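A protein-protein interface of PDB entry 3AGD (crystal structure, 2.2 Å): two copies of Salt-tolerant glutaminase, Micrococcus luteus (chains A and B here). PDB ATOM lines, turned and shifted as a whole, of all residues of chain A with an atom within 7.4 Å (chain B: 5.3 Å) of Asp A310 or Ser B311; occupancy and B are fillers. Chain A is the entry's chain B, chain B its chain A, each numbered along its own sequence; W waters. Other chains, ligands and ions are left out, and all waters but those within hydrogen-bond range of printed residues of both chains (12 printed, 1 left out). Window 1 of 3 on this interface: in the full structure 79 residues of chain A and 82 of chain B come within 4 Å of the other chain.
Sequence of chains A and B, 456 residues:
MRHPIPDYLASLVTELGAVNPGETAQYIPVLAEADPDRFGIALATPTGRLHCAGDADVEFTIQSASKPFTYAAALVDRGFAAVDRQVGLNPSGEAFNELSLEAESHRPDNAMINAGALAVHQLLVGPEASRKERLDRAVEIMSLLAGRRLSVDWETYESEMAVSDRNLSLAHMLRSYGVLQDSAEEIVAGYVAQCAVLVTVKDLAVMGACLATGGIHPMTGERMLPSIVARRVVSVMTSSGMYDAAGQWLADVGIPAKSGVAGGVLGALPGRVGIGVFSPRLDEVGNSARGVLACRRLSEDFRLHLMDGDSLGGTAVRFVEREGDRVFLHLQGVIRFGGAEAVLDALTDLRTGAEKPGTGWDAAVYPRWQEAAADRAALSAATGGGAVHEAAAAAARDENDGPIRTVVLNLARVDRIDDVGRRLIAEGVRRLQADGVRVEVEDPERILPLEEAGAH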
ATOM      1  N   PRO A  46     -30.633  31.361  21.647  1.00  0.00           N
ATOM      2  CA  PRO A  46     -29.838  30.666  22.664  1.00  0.00           C
ATOM      3  C   PRO A  46     -29.335  31.679  23.697  1.00  0.00           C
ATOM      4  O   PRO A  46     -28.916  31.315  24.796  1.00  0.00           O
ATOM      5  CB  PRO A  46     -28.689  30.062  21.856  1.00  0.00           C
ATOM      6  CG  PRO A  46     -29.270  29.906  20.491  1.00  0.00           C
ATOM      7  CD  PRO A  46     -30.025  31.196  20.318  1.00  0.00           C
ATOM      8  N   ALA A 212     -33.369  23.479  18.941  1.00  0.00           N
ATOM      9  CA  ALA A 212     -32.285  24.147  18.232  1.00  0.00           C
ATOM     10  C   ALA A 212     -30.962  24.172  18.991  1.00  0.00           C
ATOM     11  O   ALA A 212     -29.894  24.160  18.376  1.00  0.00           O
ATOM     12  CB  ALA A 212     -32.703  25.568  17.876  1.00  0.00           C
ATOM     13  N   LEU A 269     -33.897  25.974  14.018  1.00  0.00           N
ATOM     14  CA  LEU A 269     -32.637  26.031  13.294  1.00  0.00           C
ATOM     15  C   LEU A 269     -31.494  25.810  14.284  1.00  0.00           C
ATOM     16  O   LEU A 269     -31.173  26.686  15.088  1.00  0.00           O
ATOM     17  CB  LEU A 269     -32.505  27.386  12.594  1.00  0.00           C
ATOM     18  CG  LEU A 269     -31.267  27.576  11.715  1.00  0.00           C
ATOM     19  CD1 LEU A 269     -31.268  26.542  10.588  1.00  0.00           C
ATOM     20  CD2 LEU A 269     -31.266  28.982  11.146  1.00  0.00           C
ATOM     21  N   PRO A 270     -30.862  24.626  14.232  1.00  0.00           N
ATOM     22  CA  PRO A 270     -29.755  24.264  15.124  1.00  0.00           C
ATOM     23  C   PRO A 270     -28.710  25.353  15.347  1.00  0.00           C
ATOM     24  O   PRO A 270     -28.214  25.965  14.398  1.00  0.00           O
ATOM     25  CB  PRO A 270     -29.168  23.021  14.459  1.00  0.00           C
ATOM     26  CG  PRO A 270     -30.381  22.385  13.840  1.00  0.00           C
ATOM     27  CD  PRO A 270     -31.076  23.577  13.217  1.00  0.00           C
ATOM     28  N   GLY A 271     -28.385  25.569  16.618  1.00  0.00           N
ATOM     29  CA  GLY A 271     -27.396  26.558  17.003  1.00  0.00           C
ATOM     30  C   GLY A 271     -27.799  28.013  16.855  1.00  0.00           C
ATOM     31  O   GLY A 271     -27.005  28.900  17.158  1.00  0.00           O
ATOM     32  N   ARG A 272     -29.019  28.292  16.412  1.00  0.00           N
ATOM     33  CA  ARG A 272     -29.377  29.690  16.243  1.00  0.00           C
ATOM     34  C   ARG A 272     -30.727  30.211  16.691  1.00  0.00           C
ATOM     35  O   ARG A 272     -30.783  31.228  17.381  1.00  0.00           O
ATOM     36  CB  ARG A 272     -29.112  30.084  14.796  1.00  0.00           C
ATOM     37  CG  ARG A 272     -27.619  30.177  14.553  1.00  0.00           C
ATOM     38  CD  ARG A 272     -27.285  30.195  13.118  1.00  0.00           C
ATOM     39  NE  ARG A 272     -27.486  28.897  12.494  1.00  0.00           N
ATOM     40  CZ  ARG A 272     -27.469  28.734  11.181  1.00  0.00           C
ATOM     41  NH1 ARG A 272     -27.260  29.792  10.413  1.00  0.00           N
ATOM     42  NH2 ARG A 272     -27.674  27.540  10.638  1.00  0.00           N
ATOM     43  N   LEU A 304     -30.460  32.890   6.833  1.00  0.00           N
ATOM     44  CA  LEU A 304     -30.428  31.758   7.743  1.00  0.00           C
ATOM     45  C   LEU A 304     -30.640  30.480   6.940  1.00  0.00           C
ATOM     46  O   LEU A 304     -31.493  30.429   6.050  1.00  0.00           O
ATOM     47  CB  LEU A 304     -31.526  31.897   8.799  1.00  0.00           C
ATOM     48  CG  LEU A 304     -31.346  33.009   9.836  1.00  0.00           C
ATOM     49  CD1 LEU A 304     -32.634  33.184  10.608  1.00  0.00           C
ATOM     50  CD2 LEU A 304     -30.185  32.665  10.775  1.00  0.00           C
ATOM     51  N   HIS A 305     -29.855  29.453   7.243  1.00  0.00           N
ATOM     52  CA  HIS A 305     -29.986  28.193   6.537  1.00  0.00           C
ATOM     53  C   HIS A 305     -29.277  27.082   7.289  1.00  0.00           C
ATOM     54  O   HIS A 305     -28.228  27.291   7.901  1.00  0.00           O
ATOM     55  CB  HIS A 305     -29.414  28.316   5.117  1.00  0.00           C
ATOM     56  CG  HIS A 305     -29.915  27.262   4.176  1.00  0.00           C
ATOM     57  ND1 HIS A 305     -29.543  25.939   4.275  1.00  0.00           N
ATOM     58  CD2 HIS A 305     -30.796  27.333   3.151  1.00  0.00           C
ATOM     59  CE1 HIS A 305     -30.179  25.237   3.350  1.00  0.00           C
ATOM     60  NE2 HIS A 305     -30.944  26.059   2.657  1.00  0.00           N
ATOM     61  N   LEU A 306     -29.871  25.897   7.255  1.00  0.00           N
ATOM     62  CA  LEU A 306     -29.296  24.744   7.921  1.00  0.00           C
ATOM     63  C   LEU A 306     -27.881  24.506   7.404  1.00  0.00           C
ATOM     64  O   LEU A 306     -27.025  24.009   8.132  1.00  0.00           O
ATOM     65  CB  LEU A 306     -30.162  23.510   7.645  1.00  0.00           C
ATOM     66  CG  LEU A 306     -29.778  22.177   8.293  1.00  0.00           C
ATOM     67  CD1 LEU A 306     -29.767  22.303   9.813  1.00  0.00           C
ATOM     68  CD2 LEU A 306     -30.777  21.109   7.857  1.00  0.00           C
ATOM     69  N   MET A 307     -27.642  24.885   6.150  1.00  0.00           N
ATOM     70  CA  MET A 307     -26.346  24.682   5.507  1.00  0.00           C
ATOM     71  C   MET A 307     -25.289  25.755   5.717  1.00  0.00           C
ATOM     72  O   MET A 307     -24.133  25.532   5.370  1.00  0.00           O
ATOM     73  CB  MET A 307     -26.519  24.506   3.996  1.00  0.00           C
ATOM     74  CG  MET A 307     -27.435  23.377   3.569  1.00  0.00           C
ATOM     75  SD  MET A 307     -26.957  21.778   4.210  1.00  0.00           S
ATOM     76  CE  MET A 307     -28.543  21.128   4.642  1.00  0.00           C
ATOM     77  N   ASP A 308     -25.649  26.916   6.253  1.00  0.00           N
ATOM     78  CA  ASP A 308     -24.624  27.941   6.424  1.00  0.00           C
ATOM     79  C   ASP A 308     -23.600  27.522   7.486  1.00  0.00           C
ATOM     80  O   ASP A 308     -23.954  27.095   8.583  1.00  0.00           O
ATOM     81  CB  ASP A 308     -25.266  29.318   6.702  1.00  0.00           C
ATOM     82  CG  ASP A 308     -26.142  29.331   7.923  1.00  0.00           C
ATOM     83  OD1 ASP A 308     -27.050  30.192   7.989  1.00  0.00           O
ATOM     84  OD2 ASP A 308     -25.917  28.494   8.821  1.00  0.00           O
ATOM     85  N   GLY A 309     -22.322  27.617   7.125  1.00  0.00           N
ATOM     86  CA  GLY A 309     -21.248  27.204   8.016  1.00  0.00           C
ATOM     87  C   GLY A 309     -20.837  28.125   9.149  1.00  0.00           C
ATOM     88  O   GLY A 309     -19.679  28.534   9.235  1.00  0.00           O
ATOM     89  N   ASP A 310     -21.779  28.430  10.032  1.00  0.00           N
ATOM     90  CA  ASP A 310     -21.524  29.299  11.177  1.00  0.00           C
ATOM     91  C   ASP A 310     -21.086  28.443  12.373  1.00  0.00           C
ATOM     92  O   ASP A 310     -21.912  28.073  13.207  1.00  0.00           O
ATOM     93  CB  ASP A 310     -22.806  30.064  11.523  1.00  0.00           C
ATOM     94  CG  ASP A 310     -22.620  31.034  12.667  1.00  0.00           C
ATOM     95  OD1 ASP A 310     -21.941  30.675  13.654  1.00  0.00           O
ATOM     96  OD2 ASP A 310     -23.168  32.154  12.583  1.00  0.00           O
ATOM     97  N   SER A 311     -19.798  28.120  12.455  1.00  0.00           N
ATOM     98  CA  SER A 311     -19.296  27.300  13.558  1.00  0.00           C
ATOM     99  C   SER A 311     -18.227  28.019  14.367  1.00  0.00           C
ATOM    100  O   SER A 311     -17.633  28.990  13.901  1.00  0.00           O
ATOM    101  CB  SER A 311     -18.717  25.986  13.028  1.00  0.00           C
ATOM    102  OG  SER A 311     -19.702  25.218  12.359  1.00  0.00           O
ATOM    103  N   LEU A 312     -17.982  27.535  15.581  1.00  0.00           N
ATOM    104  CA  LEU A 312     -16.972  28.131  16.446  1.00  0.00           C
ATOM    105  C   LEU A 312     -15.599  28.012  15.785  1.00  0.00           C
ATOM    106  O   LEU A 312     -14.891  29.009  15.617  1.00  0.00           O
ATOM    107  CB  LEU A 312     -16.960  27.436  17.807  1.00  0.00           C
ATOM    108  CG  LEU A 312     -15.881  27.888  18.798  1.00  0.00           C
ATOM    109  CD1 LEU A 312     -15.989  29.389  19.059  1.00  0.00           C
ATOM    110  CD2 LEU A 312     -16.035  27.108  20.089  1.00  0.00           C
ATOM    111  N   GLY A 313     -15.233  26.791  15.407  1.00  0.00           N
ATOM    112  CA  GLY A 313     -13.953  26.563  14.758  1.00  0.00           C
ATOM    113  C   GLY A 313     -12.741  27.084  15.510  1.00  0.00           C
ATOM    114  O   GLY A 313     -12.611  26.883  16.720  1.00  0.00           O
ATOM    115  N   GLY A 333     -15.770  29.469  24.317  1.00  0.00           N
ATOM    116  CA  GLY A 333     -16.906  28.989  23.544  1.00  0.00           C
ATOM    117  C   GLY A 333     -17.445  27.601  23.847  1.00  0.00           C
ATOM    118  O   GLY A 333     -17.099  26.984  24.849  1.00  0.00           O
ATOM    119  N   VAL A 334     -18.322  27.129  22.965  1.00  0.00           N
ATOM    120  CA  VAL A 334     -18.937  25.810  23.074  1.00  0.00           C
ATOM    121  C   VAL A 334     -18.075  24.865  22.246  1.00  0.00           C
ATOM    122  O   VAL A 334     -18.224  24.785  21.025  1.00  0.00           O
ATOM    123  CB  VAL A 334     -20.359  25.820  22.490  1.00  0.00           C
ATOM    124  CG1 VAL A 334     -20.940  24.420  22.510  1.00  0.00           C
ATOM    125  CG2 VAL A 334     -21.232  26.783  23.276  1.00  0.00           C
ATOM    126  N   ARG A 336     -16.709  21.431  20.710  1.00  0.00           N
ATOM    127  CA  ARG A 336     -17.091  20.093  20.268  1.00  0.00           C
ATOM    128  C   ARG A 336     -15.989  19.669  19.300  1.00  0.00           C
ATOM    129  O   ARG A 336     -14.864  20.159  19.413  1.00  0.00           O
ATOM    130  CB  ARG A 336     -18.455  20.124  19.578  1.00  0.00           C
ATOM    131  CG  ARG A 336     -19.568  20.652  20.476  1.00  0.00           C
ATOM    132  CD  ARG A 336     -20.949  20.341  19.916  1.00  0.00           C
ATOM    133  NE  ARG A 336     -21.177  18.902  19.824  1.00  0.00           N
ATOM    134  CZ  ARG A 336     -22.286  18.344  19.349  1.00  0.00           C
ATOM    135  NH1 ARG A 336     -23.281  19.107  18.923  1.00  0.00           N
ATOM    136  NH2 ARG A 336     -22.394  17.022  19.290  1.00  0.00           N
ATOM    137  N   GLY B 271     -19.359  24.101   7.787  1.00  0.00           N
ATOM    138  CA  GLY B 271     -18.659  24.708   8.901  1.00  0.00           C
ATOM    139  C   GLY B 271     -17.654  23.845   9.633  1.00  0.00           C
ATOM    140  O   GLY B 271     -16.985  24.330  10.545  1.00  0.00           O
ATOM    141  N   GLY B 309     -25.709  22.245  17.194  1.00  0.00           N
ATOM    142  CA  GLY B 309     -25.676  23.689  17.344  1.00  0.00           C
ATOM    143  C   GLY B 309     -24.306  24.279  17.600  1.00  0.00           C
ATOM    144  O   GLY B 309     -24.129  25.070  18.523  1.00  0.00           O
ATOM    145  N   ASP B 310     -23.335  23.899  16.779  1.00  0.00           N
ATOM    146  CA  ASP B 310     -21.978  24.403  16.928  1.00  0.00           C
ATOM    147  C   ASP B 310     -21.890  25.782  16.272  1.00  0.00           C
ATOM    148  O   ASP B 310     -21.315  25.929  15.191  1.00  0.00           O
ATOM    149  CB  ASP B 310     -20.991  23.441  16.259  1.00  0.00           C
ATOM    150  CG  ASP B 310     -19.549  23.823  16.505  1.00  0.00           C
ATOM    151  OD1 ASP B 310     -19.251  25.039  16.541  1.00  0.00           O
ATOM    152  OD2 ASP B 310     -18.711  22.910  16.652  1.00  0.00           O
ATOM    153  N   SER B 311     -22.471  26.788  16.917  1.00  0.00           N
ATOM    154  CA  SER B 311     -22.449  28.138  16.368  1.00  0.00           C
ATOM    155  C   SER B 311     -21.684  29.111  17.248  1.00  0.00           C
ATOM    156  O   SER B 311     -21.566  28.908  18.453  1.00  0.00           O
ATOM    157  CB  SER B 311     -23.873  28.656  16.171  1.00  0.00           C
ATOM    158  OG  SER B 311     -24.569  27.864  15.229  1.00  0.00           O
ATOM    159  N   LEU B 312     -21.159  30.166  16.632  1.00  0.00           N
ATOM    160  CA  LEU B 312     -20.417  31.184  17.364  1.00  0.00           C
ATOM    161  C   LEU B 312     -21.313  31.739  18.459  1.00  0.00           C
ATOM    162  O   LEU B 312     -20.937  31.769  19.632  1.00  0.00           O
ATOM    163  CB  LEU B 312     -20.004  32.322  16.430  1.00  0.00           C
ATOM    164  CG  LEU B 312     -19.249  33.465  17.117  1.00  0.00           C
ATOM    165  CD1 LEU B 312     -17.962  32.924  17.733  1.00  0.00           C
ATOM    166  CD2 LEU B 312     -18.950  34.562  16.113  1.00  0.00           C
ATOM    167  N   GLY B 313     -22.503  32.178  18.058  1.00  0.00           N
ATOM    168  CA  GLY B 313     -23.456  32.727  19.004  1.00  0.00           C
ATOM    169  C   GLY B 313     -22.910  33.848  19.870  1.00  0.00           C
ATOM    170  O   GLY B 313     -22.284  34.786  19.370  1.00  0.00           O
ATOM    171  N   VAL B 334     -16.418  34.488  13.160  1.00  0.00           N
ATOM    172  CA  VAL B 334     -17.097  34.631  11.875  1.00  0.00           C
ATOM    173  C   VAL B 334     -18.510  35.089  12.210  1.00  0.00           C
ATOM    174  O   VAL B 334     -19.336  34.298  12.668  1.00  0.00           O
ATOM    175  CB  VAL B 334     -17.157  33.283  11.125  1.00  0.00           C
ATOM    176  CG1 VAL B 334     -18.108  33.376   9.942  1.00  0.00           C
ATOM    177  CG2 VAL B 334     -15.761  32.900  10.656  1.00  0.00           C
ATOM    178  N   ARG B 336     -22.255  36.310  11.489  1.00  0.00           N
ATOM    179  CA  ARG B 336     -23.399  36.272  10.591  1.00  0.00           C
ATOM    180  C   ARG B 336     -24.597  36.594  11.481  1.00  0.00           C
ATOM    181  O   ARG B 336     -24.434  37.261  12.504  1.00  0.00           O
ATOM    182  CB  ARG B 336     -23.522  34.887   9.955  1.00  0.00           C
ATOM    183  CG  ARG B 336     -22.323  34.544   9.065  1.00  0.00           C
ATOM    184  CD  ARG B 336     -22.273  33.071   8.688  1.00  0.00           C
ATOM    185  NE  ARG B 336     -22.835  32.776   7.371  1.00  0.00           N
ATOM    186  CZ  ARG B 336     -24.103  32.972   7.028  1.00  0.00           C
ATOM    187  NH1 ARG B 336     -24.952  33.476   7.907  1.00  0.00           N
ATOM    188  NH2 ARG B 336     -24.526  32.649   5.814  1.00  0.00           N
ATOM    189  N   PHE B 337     -25.791  36.135  11.125  1.00  0.00           N
ATOM    190  CA  PHE B 337     -26.952  36.441  11.954  1.00  0.00           C
ATOM    191  C   PHE B 337     -26.747  36.105  13.428  1.00  0.00           C
ATOM    192  O   PHE B 337     -26.946  36.951  14.296  1.00  0.00           O
ATOM    193  CB  PHE B 337     -28.198  35.701  11.478  1.00  0.00           C
ATOM    194  CG  PHE B 337     -29.400  35.960  12.342  1.00  0.00           C
ATOM    195  CD1 PHE B 337     -30.162  37.116  12.170  1.00  0.00           C
ATOM    196  CD2 PHE B 337     -29.726  35.091  13.380  1.00  0.00           C
ATOM    197  CE1 PHE B 337     -31.233  37.400  13.026  1.00  0.00           C
ATOM    198  CE2 PHE B 337     -30.794  35.370  14.241  1.00  0.00           C
ATOM    199  CZ  PHE B 337     -31.547  36.526  14.062  1.00  0.00           C
ATOM    200  N   GLY B 338     -26.360  34.859  13.695  1.00  0.00           N
ATOM    201  CA  GLY B 338     -26.155  34.403  15.059  1.00  0.00           C
ATOM    202  C   GLY B 338     -25.313  35.292  15.952  1.00  0.00           C
ATOM    203  O   GLY B 338     -25.717  35.622  17.071  1.00  0.00           O
ATOM    204  N   GLY B 339     -24.132  35.664  15.472  1.00  0.00           N
ATOM    205  CA  GLY B 339     -23.257  36.516  16.255  1.00  0.00           C
ATOM    206  C   GLY B 339     -23.792  37.931  16.372  1.00  0.00           C
ATOM    207  O   GLY B 339     -23.707  38.544  17.435  1.00  0.00           O
HETATM  208  O   HOH W   1     -21.728  23.656  13.449  1.00  0.00           O
HETATM  209  O   HOH W   2     -24.536  21.440  19.817  1.00  0.00           O
HETATM  210  O   HOH W   3     -19.249  28.964  20.929  1.00  0.00           O
HETATM  211  O   HOH W   4     -24.378  27.851  12.376  1.00  0.00           O
HETATM  212  O   HOH W   5     -16.896  23.542  18.669  1.00  0.00           O
HETATM  213  O   HOH W   6     -26.082  32.523  11.959  1.00  0.00           O
HETATM  214  O   HOH W   7     -16.674  24.369  15.347  1.00  0.00           O
HETATM  215  O   HOH W   8     -16.353  31.829  14.418  1.00  0.00           O
HETATM  216  O   HOH W   9     -27.954  21.492  18.580  1.00  0.00           O
HETATM  217  O   HOH W  10     -20.929  30.551   6.695  1.00  0.00           O
HETATM  218  O   HOH W  11     -24.141  32.109  15.413  1.00  0.00           O
HETATM  219  O   HOH W  12     -22.112  34.287  13.631  1.00  0.00           O
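Among the printed residues, pairs that only touch across the chains: Gly A271 with Gly B309, Leu A304 with Phe B337, Gly A309 with Gly B271, Asp A310 with Arg B336, Arg A272 with Ser B311 and Pro A270 with Gly B309.
Water W12 lies within hydrogen-bond range of the side-chain carboxylate (OD2) of Asp A310 (2.6 Å), the backbone carbonyl oxygen (O) of Val B334 (2.9 Å), the backbone NH (N) of Arg B336 (2.9 Å) and the backbone NH (N) of Gly B339 (3.1 Å).
Water W4 lies within hydrogen-bond range of O of Asp A310 (2.6 Å), OG of Ser B311 (2.9 Å) and NE of Arg A272 (3.3 Å).
Water W9 bridges the backbone NH of Gly B309 (2.7 Å) and the backbone carbonyl oxygen of Ala A212 (3.3 Å).
Water W5 lies within hydrogen-bond range of OD2 of Asp B310 (2.8 Å), N of Arg A336 (2.9 Å) and O of Val A334 (3.0 Å).
Water W3 lies within hydrogen-bond range of the backbone NH (N) of Val A334 (2.9 Å) and the backbone carbonyl oxygen (O) of Ser B311 (3.4 Å).
Water W10 lies within hydrogen-bond range of the guanidinium group (NE) of Arg B336 (3.0 Å) and the backbone NH (N) of Gly A309 (3.3 Å).
Gly A271 touches Gly B309, and with the chains exchanged Gly A309 touches Gly B271.
Gly A271 touches Ser B311, and with the chains exchanged Ser A311 touches Gly B271.
Asp A310 touches Ser B311, and with the chains exchanged Ser A311 touches Asp B310.
Asp A310 touches Arg B336, but with the chains exchanged Arg A336 does not touch Asp B310 (4.05 Å).
Positions printed for both chains: 271, 309, 310, 311, 312, 313, 334 and 336.
Of the 14 pairs that touch across the chains among the printed residues, 9 have their exchanged pair printed and touching as well.
Printed residues of chain B within 4 Å of Pro A270: Gly B309 (3.995 Å).
Of the printed residues of chain B, Gly A271 touches Gly B309 (3.4 Å) and Ser B311 (3.3 Å).
Ser B311 touches just these residues of chain A: Gly A271 (3.3 Å), Arg A272 (3.9 Å) and Asp A310 (3.2 Å).
Of the 19 printed residues of chain A, 9 touch a printed residue of chain B.
Hydrophobic or aromatic side chains of chain A that line the printed part of chain B: Leu A304 and Leu A312.
Along chain A the printed residues that touch a printed residue of chain B span positions 270 to 312.
Among the printed residues, Asp or Glu carboxylates within 4 Å of a Lys or Arg side-chain nitrogen of the other chain: Asp A308 with Arg B336.
The backbone carbonyl oxygen (O) of Asp A310 sits close to the backbone carbonyl oxygen (O) of Asp B310, at 3.0 Å.
The side-chain hydroxyl of Ser B311 lies close to the backbone carbonyl oxygen of Asp A310, 3.3 Å away.
The side-chain hydroxyl (OG) of Ser B311 is in hydrogen-bond range of the backbone carbonyl oxygen (O) of Gly A271 (3.3 Å).
O of Asp B310 sits close to OG of Ser A311 (3.3 Å).
The guanidinium group (NH1) of Arg B336 lies within salt-bridge range of the side-chain carboxylate (OD1) of Asp A308 (3.9 Å).
O of Gly B271 lies within hydrogen-bond range of OG of Ser A311 (3.4 Å).
OD1 of Asp B310 sits at hydrogen-bond distance from N of Leu A312 (3.0 Å).
OD1 of Asp A310 is in hydrogen-bond range of N of Leu B312 (3.1 Å).
O of His A305 sits at hydrogen-bond distance from NH2 of Arg A272, at 2.8 Å.
The backbone carbonyl oxygen (O) of Ala A212 lies within hydrogen-bond range of the backbone NH (N) of Gly A271 (2.7 Å).
The side-chain carboxylate (OD1) of Asp A308 is in hydrogen-bond range of the backbone NH (N) of His A305 (3.0 Å).
The guanidinium group (NH1) of Arg A272 lies within salt-bridge range of the side-chain carboxylate (OD2) of Asp A308 (2.5 Å).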
